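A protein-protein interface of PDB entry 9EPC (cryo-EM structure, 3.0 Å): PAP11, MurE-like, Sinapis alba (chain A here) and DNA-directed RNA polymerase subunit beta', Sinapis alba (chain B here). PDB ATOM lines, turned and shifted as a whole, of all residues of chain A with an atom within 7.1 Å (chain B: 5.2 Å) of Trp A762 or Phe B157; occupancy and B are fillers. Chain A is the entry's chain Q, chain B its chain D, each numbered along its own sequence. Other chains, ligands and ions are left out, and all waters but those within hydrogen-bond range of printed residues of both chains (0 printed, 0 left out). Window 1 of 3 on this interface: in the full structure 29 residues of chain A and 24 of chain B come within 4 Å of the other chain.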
ATOM      1  N   TYR A 682     -24.079 -15.844  -0.950  1.00  0.00           N
ATOM      2  CA  TYR A 682     -24.754 -17.108  -0.705  1.00  0.00           C
ATOM      3  C   TYR A 682     -25.973 -17.199  -1.602  1.00  0.00           C
ATOM      4  O   TYR A 682     -26.895 -16.381  -1.459  1.00  0.00           O
ATOM      5  CB  TYR A 682     -25.158 -17.225   0.757  1.00  0.00           C
ATOM      6  CG  TYR A 682     -24.002 -17.044   1.709  1.00  0.00           C
ATOM      7  CD1 TYR A 682     -23.101 -18.073   1.936  1.00  0.00           C
ATOM      8  CD2 TYR A 682     -23.808 -15.845   2.376  1.00  0.00           C
ATOM      9  CE1 TYR A 682     -22.042 -17.913   2.803  1.00  0.00           C
ATOM     10  CE2 TYR A 682     -22.751 -15.676   3.246  1.00  0.00           C
ATOM     11  CZ  TYR A 682     -21.871 -16.714   3.454  1.00  0.00           C
ATOM     12  OH  TYR A 682     -20.815 -16.552   4.320  1.00  0.00           O
ATOM     13  N   LEU A 693     -26.028 -19.769   7.658  1.00  0.00           N
ATOM     14  CA  LEU A 693     -25.676 -20.517   8.855  1.00  0.00           C
ATOM     15  C   LEU A 693     -24.441 -19.929   9.527  1.00  0.00           C
ATOM     16  O   LEU A 693     -23.528 -19.429   8.868  1.00  0.00           O
ATOM     17  CB  LEU A 693     -25.441 -21.990   8.523  1.00  0.00           C
ATOM     18  CG  LEU A 693     -24.224 -22.360   7.676  1.00  0.00           C
ATOM     19  CD1 LEU A 693     -23.064 -22.806   8.550  1.00  0.00           C
ATOM     20  CD2 LEU A 693     -24.582 -23.437   6.673  1.00  0.00           C
ATOM     21  N   HIS A 694     -24.427 -19.992  10.858  1.00  0.00           N
ATOM     22  CA  HIS A 694     -23.259 -19.589  11.631  1.00  0.00           C
ATOM     23  C   HIS A 694     -23.203 -20.430  12.895  1.00  0.00           C
ATOM     24  O   HIS A 694     -24.192 -20.515  13.628  1.00  0.00           O
ATOM     25  CB  HIS A 694     -23.304 -18.102  11.982  1.00  0.00           C
ATOM     26  CG  HIS A 694     -21.967 -17.528  12.327  1.00  0.00           C
ATOM     27  ND1 HIS A 694     -21.214 -17.982  13.388  1.00  0.00           N
ATOM     28  CD2 HIS A 694     -21.243 -16.545  11.746  1.00  0.00           C
ATOM     29  CE1 HIS A 694     -20.083 -17.301  13.445  1.00  0.00           C
ATOM     30  NE2 HIS A 694     -20.077 -16.420  12.462  1.00  0.00           N
ATOM     31  N   VAL A 699     -23.372 -14.897  18.241  1.00  0.00           N
ATOM     32  CA  VAL A 699     -23.248 -14.022  17.086  1.00  0.00           C
ATOM     33  C   VAL A 699     -24.278 -14.353  16.020  1.00  0.00           C
ATOM     34  O   VAL A 699     -24.344 -13.665  14.997  1.00  0.00           O
ATOM     35  CB  VAL A 699     -21.828 -14.094  16.499  1.00  0.00           C
ATOM     36  CG1 VAL A 699     -20.799 -14.157  17.614  1.00  0.00           C
ATOM     37  CG2 VAL A 699     -21.701 -15.286  15.574  1.00  0.00           C
ATOM     38  N   ALA A 700     -25.087 -15.389  16.230  1.00  0.00           N
ATOM     39  CA  ALA A 700     -26.099 -15.770  15.251  1.00  0.00           C
ATOM     40  C   ALA A 700     -27.458 -15.157  15.565  1.00  0.00           C
ATOM     41  O   ALA A 700     -28.099 -14.584  14.682  1.00  0.00           O
ATOM     42  CB  ALA A 700     -26.212 -17.293  15.181  1.00  0.00           C
ATOM     43  N   ARG A 702     -28.051 -12.557  17.518  1.00  0.00           N
ATOM     44  CA  ARG A 702     -27.904 -11.116  17.361  1.00  0.00           C
ATOM     45  C   ARG A 702     -27.855 -10.728  15.890  1.00  0.00           C
ATOM     46  O   ARG A 702     -28.426  -9.708  15.491  1.00  0.00           O
ATOM     47  CB  ARG A 702     -26.649 -10.632  18.083  1.00  0.00           C
ATOM     48  CG  ARG A 702     -26.670 -10.858  19.581  1.00  0.00           C
ATOM     49  CD  ARG A 702     -25.342 -10.482  20.202  1.00  0.00           C
ATOM     50  NE  ARG A 702     -25.342 -10.672  21.647  1.00  0.00           N
ATOM     51  CZ  ARG A 702     -25.581  -9.711  22.527  1.00  0.00           C
ATOM     52  NH1 ARG A 702     -25.835  -8.471  22.144  1.00  0.00           N
ATOM     53  NH2 ARG A 702     -25.566 -10.001  23.824  1.00  0.00           N
ATOM     54  N   CYS A 703     -27.178 -11.531  15.069  1.00  0.00           N
ATOM     55  CA  CYS A 703     -27.092 -11.226  13.644  1.00  0.00           C
ATOM     56  C   CYS A 703     -28.460 -11.292  12.979  1.00  0.00           C
ATOM     57  O   CYS A 703     -28.775 -10.466  12.115  1.00  0.00           O
ATOM     58  CB  CYS A 703     -26.120 -12.181  12.958  1.00  0.00           C
ATOM     59  SG  CYS A 703     -25.847 -11.830  11.213  1.00  0.00           S
ATOM     60  N   ALA A 704     -29.282 -12.271  13.360  1.00  0.00           N
ATOM     61  CA  ALA A 704     -30.612 -12.386  12.770  1.00  0.00           C
ATOM     62  C   ALA A 704     -31.482 -11.192  13.138  1.00  0.00           C
ATOM     63  O   ALA A 704     -32.318 -10.756  12.339  1.00  0.00           O
ATOM     64  CB  ALA A 704     -31.274 -13.688  13.213  1.00  0.00           C
ATOM     65  N   ALA A 706     -30.480  -8.076  13.552  1.00  0.00           N
ATOM     66  CA  ALA A 706     -30.100  -6.981  12.670  1.00  0.00           C
ATOM     67  C   ALA A 706     -30.561  -7.203  11.237  1.00  0.00           C
ATOM     68  O   ALA A 706     -30.560  -6.256  10.445  1.00  0.00           O
ATOM     69  CB  ALA A 706     -28.585  -6.782  12.702  1.00  0.00           C
ATOM     70  N   MET A 707     -30.957  -8.423  10.890  1.00  0.00           N
ATOM     71  CA  MET A 707     -31.363  -8.759   9.535  1.00  0.00           C
ATOM     72  C   MET A 707     -32.828  -8.451   9.261  1.00  0.00           C
ATOM     73  O   MET A 707     -33.285  -8.643   8.130  1.00  0.00           O
ATOM     74  CB  MET A 707     -31.090 -10.240   9.265  1.00  0.00           C
ATOM     75  CG  MET A 707     -30.576 -10.536   7.875  1.00  0.00           C
ATOM     76  SD  MET A 707     -29.932 -12.213   7.748  1.00  0.00           S
ATOM     77  CE  MET A 707     -28.764 -12.219   9.104  1.00  0.00           C
ATOM     78  N   LEU A 750     -25.337   0.054  14.684  1.00  0.00           N
ATOM     79  CA  LEU A 750     -24.712  -0.632  13.560  1.00  0.00           C
ATOM     80  C   LEU A 750     -25.119   0.003  12.237  1.00  0.00           C
ATOM     81  O   LEU A 750     -24.281   0.199  11.350  1.00  0.00           O
ATOM     82  CB  LEU A 750     -25.081  -2.113  13.587  1.00  0.00           C
ATOM     83  CG  LEU A 750     -24.082  -3.061  12.929  1.00  0.00           C
ATOM     84  CD1 LEU A 750     -22.707  -2.856  13.527  1.00  0.00           C
ATOM     85  CD2 LEU A 750     -24.528  -4.498  13.106  1.00  0.00           C
ATOM     86  N   ILE A 755     -23.109   0.037   8.371  1.00  0.00           N
ATOM     87  CA  ILE A 755     -23.076  -1.409   8.193  1.00  0.00           C
ATOM     88  C   ILE A 755     -24.385  -1.860   7.562  1.00  0.00           C
ATOM     89  O   ILE A 755     -25.470  -1.567   8.077  1.00  0.00           O
ATOM     90  CB  ILE A 755     -22.836  -2.118   9.535  1.00  0.00           C
ATOM     91  CG1 ILE A 755     -21.748  -1.399  10.335  1.00  0.00           C
ATOM     92  CG2 ILE A 755     -22.458  -3.566   9.306  1.00  0.00           C
ATOM     93  CD1 ILE A 755     -20.414  -1.326   9.638  1.00  0.00           C
ATOM     94  N   ASP A 756     -24.288  -2.573   6.442  1.00  0.00           N
ATOM     95  CA  ASP A 756     -25.467  -3.052   5.721  1.00  0.00           C
ATOM     96  C   ASP A 756     -25.761  -4.475   6.175  1.00  0.00           C
ATOM     97  O   ASP A 756     -25.230  -5.446   5.636  1.00  0.00           O
ATOM     98  CB  ASP A 756     -25.245  -2.978   4.216  1.00  0.00           C
ATOM     99  CG  ASP A 756     -26.457  -3.428   3.425  1.00  0.00           C
ATOM    100  OD1 ASP A 756     -27.556  -3.523   4.011  1.00  0.00           O
ATOM    101  OD2 ASP A 756     -26.311  -3.692   2.213  1.00  0.00           O
ATOM    102  N   THR A 757     -26.622  -4.599   7.179  1.00  0.00           N
ATOM    103  CA  THR A 757     -27.004  -5.903   7.716  1.00  0.00           C
ATOM    104  C   THR A 757     -28.334  -6.363   7.121  1.00  0.00           C
ATOM    105  O   THR A 757     -29.327  -6.562   7.819  1.00  0.00           O
ATOM    106  CB  THR A 757     -27.073  -5.845   9.237  1.00  0.00           C
ATOM    107  OG1 THR A 757     -28.145  -4.982   9.631  1.00  0.00           O
ATOM    108  CG2 THR A 757     -25.775  -5.305   9.798  1.00  0.00           C
ATOM    109  N   SER A 758     -28.338  -6.536   5.802  1.00  0.00           N
ATOM    110  CA  SER A 758     -29.499  -7.047   5.086  1.00  0.00           C
ATOM    111  C   SER A 758     -29.335  -8.514   4.711  1.00  0.00           C
ATOM    112  O   SER A 758     -30.252  -9.315   4.911  1.00  0.00           O
ATOM    113  CB  SER A 758     -29.755  -6.211   3.827  1.00  0.00           C
ATOM    114  OG  SER A 758     -28.640  -6.254   2.956  1.00  0.00           O
ATOM    115  N   GLU A 759     -28.186  -8.873   4.159  1.00  0.00           N
ATOM    116  CA  GLU A 759     -27.816 -10.258   3.924  1.00  0.00           C
ATOM    117  C   GLU A 759     -26.656 -10.635   4.836  1.00  0.00           C
ATOM    118  O   GLU A 759     -26.083  -9.792   5.529  1.00  0.00           O
ATOM    119  CB  GLU A 759     -27.452 -10.473   2.453  1.00  0.00           C
ATOM    120  CG  GLU A 759     -26.544  -9.401   1.885  1.00  0.00           C
ATOM    121  CD  GLU A 759     -26.474  -9.441   0.373  1.00  0.00           C
ATOM    122  OE1 GLU A 759     -27.033 -10.386  -0.222  1.00  0.00           O
ATOM    123  OE2 GLU A 759     -25.864  -8.527  -0.221  1.00  0.00           O
ATOM    124  N   PHE A 760     -26.324 -11.924   4.845  1.00  0.00           N
ATOM    125  CA  PHE A 760     -25.267 -12.393   5.738  1.00  0.00           C
ATOM    126  C   PHE A 760     -23.916 -11.753   5.454  1.00  0.00           C
ATOM    127  O   PHE A 760     -23.241 -11.343   6.414  1.00  0.00           O
ATOM    128  CB  PHE A 760     -25.175 -13.920   5.692  1.00  0.00           C
ATOM    129  CG  PHE A 760     -24.651 -14.519   6.958  1.00  0.00           C
ATOM    130  CD1 PHE A 760     -25.134 -14.093   8.183  1.00  0.00           C
ATOM    131  CD2 PHE A 760     -23.670 -15.491   6.934  1.00  0.00           C
ATOM    132  CE1 PHE A 760     -24.661 -14.635   9.355  1.00  0.00           C
ATOM    133  CE2 PHE A 760     -23.190 -16.037   8.106  1.00  0.00           C
ATOM    134  CZ  PHE A 760     -23.686 -15.606   9.318  1.00  0.00           C
ATOM    135  N   PRO A 761     -23.452 -11.628   4.202  1.00  0.00           N
ATOM    136  CA  PRO A 761     -22.179 -10.930   3.981  1.00  0.00           C
ATOM    137  C   PRO A 761     -22.328  -9.431   4.176  1.00  0.00           C
ATOM    138  O   PRO A 761     -22.571  -8.691   3.218  1.00  0.00           O
ATOM    139  CB  PRO A 761     -21.826 -11.286   2.533  1.00  0.00           C
ATOM    140  CG  PRO A 761     -23.128 -11.568   1.895  1.00  0.00           C
ATOM    141  CD  PRO A 761     -23.962 -12.224   2.952  1.00  0.00           C
ATOM    142  N   TRP A 762     -22.213  -8.985   5.427  1.00  0.00           N
ATOM    143  CA  TRP A 762     -22.342  -7.571   5.752  1.00  0.00           C
ATOM    144  C   TRP A 762     -21.368  -6.735   4.935  1.00  0.00           C
ATOM    145  O   TRP A 762     -20.193  -7.081   4.801  1.00  0.00           O
ATOM    146  CB  TRP A 762     -22.079  -7.348   7.240  1.00  0.00           C
ATOM    147  CG  TRP A 762     -23.120  -7.903   8.140  1.00  0.00           C
ATOM    148  CD1 TRP A 762     -24.229  -8.603   7.781  1.00  0.00           C
ATOM    149  CD2 TRP A 762     -23.154  -7.796   9.564  1.00  0.00           C
ATOM    150  NE1 TRP A 762     -24.954  -8.943   8.895  1.00  0.00           N
ATOM    151  CE2 TRP A 762     -24.313  -8.459  10.004  1.00  0.00           C
ATOM    152  CE3 TRP A 762     -22.315  -7.205  10.512  1.00  0.00           C
ATOM    153  CZ2 TRP A 762     -24.655  -8.546  11.349  1.00  0.00           C
ATOM    154  CZ3 TRP A 762     -22.655  -7.294  11.844  1.00  0.00           C
ATOM    155  CH2 TRP A 762     -23.814  -7.957  12.251  1.00  0.00           C
ATOM    156  N   ARG A 763     -21.864  -5.627   4.396  1.00  0.00           N
ATOM    157  CA  ARG A 763     -21.050  -4.706   3.608  1.00  0.00           C
ATOM    158  C   ARG A 763     -20.683  -3.521   4.492  1.00  0.00           C
ATOM    159  O   ARG A 763     -21.485  -2.604   4.687  1.00  0.00           O
ATOM    160  CB  ARG A 763     -21.789  -4.264   2.352  1.00  0.00           C
ATOM    161  CG  ARG A 763     -22.066  -5.390   1.376  1.00  0.00           C
ATOM    162  CD  ARG A 763     -22.613  -4.859   0.064  1.00  0.00           C
ATOM    163  NE  ARG A 763     -22.813  -5.922  -0.910  1.00  0.00           N
ATOM    164  CZ  ARG A 763     -23.206  -5.726  -2.161  1.00  0.00           C
ATOM    165  NH1 ARG A 763     -23.448  -4.512  -2.627  1.00  0.00           N
ATOM    166  NH2 ARG A 763     -23.359  -6.774  -2.966  1.00  0.00           N
ATOM    167  N   LEU A 764     -19.468  -3.544   5.029  1.00  0.00           N
ATOM    168  CA  LEU A 764     -18.963  -2.428   5.805  1.00  0.00           C
ATOM    169  C   LEU A 764     -18.628  -1.266   4.872  1.00  0.00           C
ATOM    170  O   LEU A 764     -18.530  -1.446   3.658  1.00  0.00           O
ATOM    171  CB  LEU A 764     -17.727  -2.851   6.595  1.00  0.00           C
ATOM    172  CG  LEU A 764     -17.788  -4.184   7.343  1.00  0.00           C
ATOM    173  CD1 LEU A 764     -16.556  -4.358   8.210  1.00  0.00           C
ATOM    174  CD2 LEU A 764     -19.045  -4.292   8.181  1.00  0.00           C
ATOM    175  N   SER A 767     -15.041  -2.138   2.258  1.00  0.00           N
ATOM    176  CA  SER A 767     -15.393  -3.503   1.894  1.00  0.00           C
ATOM    177  C   SER A 767     -14.936  -3.756   0.462  1.00  0.00           C
ATOM    178  O   SER A 767     -14.075  -3.042  -0.061  1.00  0.00           O
ATOM    179  CB  SER A 767     -16.901  -3.734   2.086  1.00  0.00           C
ATOM    180  OG  SER A 767     -17.246  -3.715   3.457  1.00  0.00           O
ATOM    181  N   ARG B 149     -10.359 -12.412   6.502  1.00  0.00           N
ATOM    182  CA  ARG B 149     -10.638 -13.816   6.219  1.00  0.00           C
ATOM    183  C   ARG B 149      -9.413 -14.714   6.417  1.00  0.00           C
ATOM    184  O   ARG B 149      -9.006 -15.427   5.493  1.00  0.00           O
ATOM    185  CB  ARG B 149     -11.192 -13.972   4.809  1.00  0.00           C
ATOM    186  CG  ARG B 149     -12.502 -13.253   4.569  1.00  0.00           C
ATOM    187  CD  ARG B 149     -13.645 -13.926   5.302  1.00  0.00           C
ATOM    188  NE  ARG B 149     -14.925 -13.308   4.981  1.00  0.00           N
ATOM    189  CZ  ARG B 149     -15.639 -13.591   3.900  1.00  0.00           C
ATOM    190  NH1 ARG B 149     -15.227 -14.481   3.013  1.00  0.00           N
ATOM    191  NH2 ARG B 149     -16.795 -12.964   3.703  1.00  0.00           N
ATOM    192  N   PRO B 155     -17.456 -20.539   9.125  1.00  0.00           N
ATOM    193  CA  PRO B 155     -18.315 -19.497   8.551  1.00  0.00           C
ATOM    194  C   PRO B 155     -17.870 -18.102   8.960  1.00  0.00           C
ATOM    195  O   PRO B 155     -17.439 -17.871  10.092  1.00  0.00           O
ATOM    196  CB  PRO B 155     -19.700 -19.831   9.117  1.00  0.00           C
ATOM    197  CG  PRO B 155     -19.622 -21.269   9.491  1.00  0.00           C
ATOM    198  CD  PRO B 155     -18.220 -21.486   9.953  1.00  0.00           C
ATOM    199  N   THR B 156     -17.989 -17.164   8.023  1.00  0.00           N
ATOM    200  CA  THR B 156     -17.654 -15.767   8.258  1.00  0.00           C
ATOM    201  C   THR B 156     -18.738 -14.889   7.652  1.00  0.00           C
ATOM    202  O   THR B 156     -19.348 -15.243   6.641  1.00  0.00           O
ATOM    203  CB  THR B 156     -16.292 -15.393   7.656  1.00  0.00           C
ATOM    204  OG1 THR B 156     -16.275 -15.721   6.263  1.00  0.00           O
ATOM    205  CG2 THR B 156     -15.167 -16.134   8.364  1.00  0.00           C
ATOM    206  N   PHE B 157     -18.976 -13.736   8.282  1.00  0.00           N
ATOM    207  CA  PHE B 157     -20.001 -12.790   7.832  1.00  0.00           C
ATOM    208  C   PHE B 157     -19.379 -11.394   7.752  1.00  0.00           C
ATOM    209  O   PHE B 157     -19.547 -10.565   8.644  1.00  0.00           O
ATOM    210  CB  PHE B 157     -21.227 -12.832   8.766  1.00  0.00           C
ATOM    211  CG  PHE B 157     -20.931 -12.447  10.193  1.00  0.00           C
ATOM    212  CD1 PHE B 157     -20.140 -13.245  10.999  1.00  0.00           C
ATOM    213  CD2 PHE B 157     -21.463 -11.288  10.731  1.00  0.00           C
ATOM    214  CE1 PHE B 157     -19.872 -12.888  12.301  1.00  0.00           C
ATOM    215  CE2 PHE B 157     -21.196 -10.927  12.032  1.00  0.00           C
ATOM    216  CZ  PHE B 157     -20.403 -11.728  12.820  1.00  0.00           C
ATOM    217  N   LEU B 158     -18.696 -11.120   6.644  1.00  0.00           N
ATOM    218  CA  LEU B 158     -18.055  -9.832   6.413  1.00  0.00           C
ATOM    219  C   LEU B 158     -17.691  -9.736   4.943  1.00  0.00           C
ATOM    220  O   LEU B 158     -17.434 -10.751   4.290  1.00  0.00           O
ATOM    221  CB  LEU B 158     -16.799  -9.648   7.278  1.00  0.00           C
ATOM    222  CG  LEU B 158     -16.932  -9.127   8.712  1.00  0.00           C
ATOM    223  CD1 LEU B 158     -15.570  -8.893   9.335  1.00  0.00           C
ATOM    224  CD2 LEU B 158     -17.768  -7.861   8.755  1.00  0.00           C
ATOM    225  N   ARG B 159     -17.667  -8.511   4.433  1.00  0.00           N
ATOM    226  CA  ARG B 159     -17.253  -8.255   3.062  1.00  0.00           C
ATOM    227  C   ARG B 159     -15.757  -7.988   2.952  1.00  0.00           C
ATOM    228  O   ARG B 159     -15.261  -7.746   1.847  1.00  0.00           O
ATOM    229  CB  ARG B 159     -18.045  -7.073   2.490  1.00  0.00           C
ATOM    230  CG  ARG B 159     -18.094  -7.003   0.972  1.00  0.00           C
ATOM    231  CD  ARG B 159     -18.974  -8.087   0.384  1.00  0.00           C
ATOM    232  NE  ARG B 159     -19.037  -7.998  -1.068  1.00  0.00           N
ATOM    233  CZ  ARG B 159     -19.862  -8.706  -1.827  1.00  0.00           C
ATOM    234  NH1 ARG B 159     -20.723  -9.561  -1.299  1.00  0.00           N
ATOM    235  NH2 ARG B 159     -19.824  -8.551  -3.147  1.00  0.00           N
ATOM    236  N   ILE B 175     -18.749  -2.985  16.159  1.00  0.00           N
ATOM    237  CA  ILE B 175     -18.919  -4.439  16.153  1.00  0.00           C
ATOM    238  C   ILE B 175     -18.701  -5.051  17.532  1.00  0.00           C
ATOM    239  O   ILE B 175     -19.538  -5.863  17.960  1.00  0.00           O
ATOM    240  CB  ILE B 175     -18.020  -5.072  15.076  1.00  0.00           C
ATOM    241  CG1 ILE B 175     -18.477  -4.645  13.684  1.00  0.00           C
ATOM    242  CG2 ILE B 175     -18.033  -6.583  15.197  1.00  0.00           C
ATOM    243  CD1 ILE B 175     -19.847  -5.149  13.320  1.00  0.00           C
ATOM    244  N   PHE B 178     -21.789  -4.400  19.625  1.00  0.00           N
ATOM    245  CA  PHE B 178     -22.991  -5.098  19.185  1.00  0.00           C
ATOM    246  C   PHE B 178     -22.994  -6.547  19.653  1.00  0.00           C
ATOM    247  O   PHE B 178     -24.012  -7.053  20.139  1.00  0.00           O
ATOM    248  CB  PHE B 178     -23.099  -5.020  17.663  1.00  0.00           C
ATOM    249  CG  PHE B 178     -24.328  -5.674  17.105  1.00  0.00           C
ATOM    250  CD1 PHE B 178     -25.525  -4.985  17.043  1.00  0.00           C
ATOM    251  CD2 PHE B 178     -24.281  -6.970  16.628  1.00  0.00           C
ATOM    252  CE1 PHE B 178     -26.654  -5.581  16.524  1.00  0.00           C
ATOM    253  CE2 PHE B 178     -25.408  -7.571  16.109  1.00  0.00           C
ATOM    254  CZ  PHE B 178     -26.596  -6.874  16.057  1.00  0.00           C
ATOM    255  N   PHE B 179     -21.861  -7.232  19.519  1.00  0.00           N
ATOM    256  CA  PHE B 179     -21.758  -8.645  19.855  1.00  0.00           C
ATOM    257  C   PHE B 179     -21.214  -8.887  21.255  1.00  0.00           C
ATOM    258  O   PHE B 179     -20.994 -10.045  21.624  1.00  0.00           O
ATOM    259  CB  PHE B 179     -20.881  -9.368  18.833  1.00  0.00           C
ATOM    260  CG  PHE B 179     -21.501  -9.479  17.475  1.00  0.00           C
ATOM    261  CD1 PHE B 179     -22.484 -10.416  17.226  1.00  0.00           C
ATOM    262  CD2 PHE B 179     -21.095  -8.653  16.445  1.00  0.00           C
ATOM    263  CE1 PHE B 179     -23.057 -10.523  15.978  1.00  0.00           C
ATOM    264  CE2 PHE B 179     -21.663  -8.756  15.194  1.00  0.00           C
ATOM    265  CZ  PHE B 179     -22.645  -9.693  14.961  1.00  0.00           C
ATOM    266  N   PHE B 187     -15.124 -14.983  17.812  1.00  0.00           N
ATOM    267  CA  PHE B 187     -14.966 -14.994  16.365  1.00  0.00           C
ATOM    268  C   PHE B 187     -14.074 -13.866  15.865  1.00  0.00           C
ATOM    269  O   PHE B 187     -13.994 -13.645  14.652  1.00  0.00           O
ATOM    270  CB  PHE B 187     -16.334 -14.916  15.686  1.00  0.00           C
ATOM    271  CG  PHE B 187     -16.960 -13.554  15.744  1.00  0.00           C
ATOM    272  CD1 PHE B 187     -17.535 -13.090  16.913  1.00  0.00           C
ATOM    273  CD2 PHE B 187     -16.975 -12.736  14.628  1.00  0.00           C
ATOM    274  CE1 PHE B 187     -18.109 -11.839  16.968  1.00  0.00           C
ATOM    275  CE2 PHE B 187     -17.546 -11.482  14.679  1.00  0.00           C
ATOM    276  CZ  PHE B 187     -18.114 -11.034  15.850  1.00  0.00           C
ATOM    277  N   GLU B 191     -12.381 -13.413  11.683  1.00  0.00           N
ATOM    278  CA  GLU B 191     -12.642 -12.374  10.697  1.00  0.00           C
ATOM    279  C   GLU B 191     -11.421 -11.496  10.450  1.00  0.00           C
ATOM    280  O   GLU B 191     -10.996 -11.331   9.304  1.00  0.00           O
ATOM    281  CB  GLU B 191     -13.829 -11.518  11.150  1.00  0.00           C
ATOM    282  CG  GLU B 191     -15.033 -12.318  11.608  1.00  0.00           C
ATOM    283  CD  GLU B 191     -15.694 -13.079  10.478  1.00  0.00           C
ATOM    284  OE1 GLU B 191     -15.502 -12.692   9.306  1.00  0.00           O
ATOM    285  OE2 GLU B 191     -16.407 -14.064  10.763  1.00  0.00           O
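Cys A703 touches none of the printed residues of chain B.
Of the printed residues of chain B, Ala A706 touches Phe B178.
Pro A761 touches none of the printed residues of chain B.
Of chain B, only Phe B157, Leu B158, Arg B159, Ile B175 and Phe B179 come within 4 Å of Trp A762.
Of the printed residues of chain B, Ser A767 touches Arg B159.
Phe B157 touches three residues of chain A.
Of the printed residues of chain A, Phe B187 touches Val A699 (3.5 Å).
Hydrophobic or aromatic side chains of chain A within 4 Å of the printed part of chain B: Tyr A682, Leu A693, His A694, Val A699, Ala A706, Leu A750, Phe A760, Trp A762 and Leu A764.
Printed residues of chain B that touch a printed residue of chain A: Pro B155, Thr B156, Phe B157, Leu B158, Arg B159, Ile B175, Phe B178, Phe B179 and Phe B187.
Among the printed residues, 18 pairs touch across the chains.
Among the printed residues, no Asp or Glu carboxylate lies within 4 Å of a Lys or Arg side-chain nitrogen of the other chain.
The backbone carbonyl oxygen of Thr B156 lies within hydrogen-bond range of the side-chain hydroxyl of Tyr A682, at 3.0 Å.
The backbone carbonyl oxygen (O) of Trp A762 sits at hydrogen-bond distance from the backbone NH (N) of Arg B159, 2.9 Å away.
O of Phe B178 lies within hydrogen-bond range of NH1 of Arg A702 (3.1 Å).
Pro B155 touches Leu A693.
Pro B155 touches His A694 (O to NE2, 3.8 Å).
O of Val A699 touches CE1 of Phe B179, at 3.5 Å.
Phe B187 touches Val A699 (CD1 to CG1, 3.5 Å).
Ile B175 touches Leu A750.
Phe A760 touches Phe B157.
Phe B157 touches Trp A762.
Leu B158 touches Trp A762.
Trp A762 touches Ile B175.
Ser A767 touches Arg B159 (CB to CB, 3.6 Å).
The guanidinium group (NE) of Arg B149 lies within hydrogen-bond range of the side-chain hydroxyl (OG1) of Thr B156 (3.0 Å).
The backbone carbonyl oxygen (O) of Leu A750 sits close to the backbone NH (N) of Ile A755, at 3.2 Å.
The backbone carbonyl oxygen (O) of Leu A764 sits at hydrogen-bond distance from the side-chain hydroxyl (OG) of Ser A767, at 2.6 Å.
The backbone carbonyl oxygen (O) of Arg A763 sits at hydrogen-bond distance from the backbone NH (N) of Asp A756 (3.3 Å).
The side-chain hydroxyl (OG1) of Thr A757 is in hydrogen-bond range of the backbone carbonyl oxygen (O) of Ala A706, at 2.8 Å.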
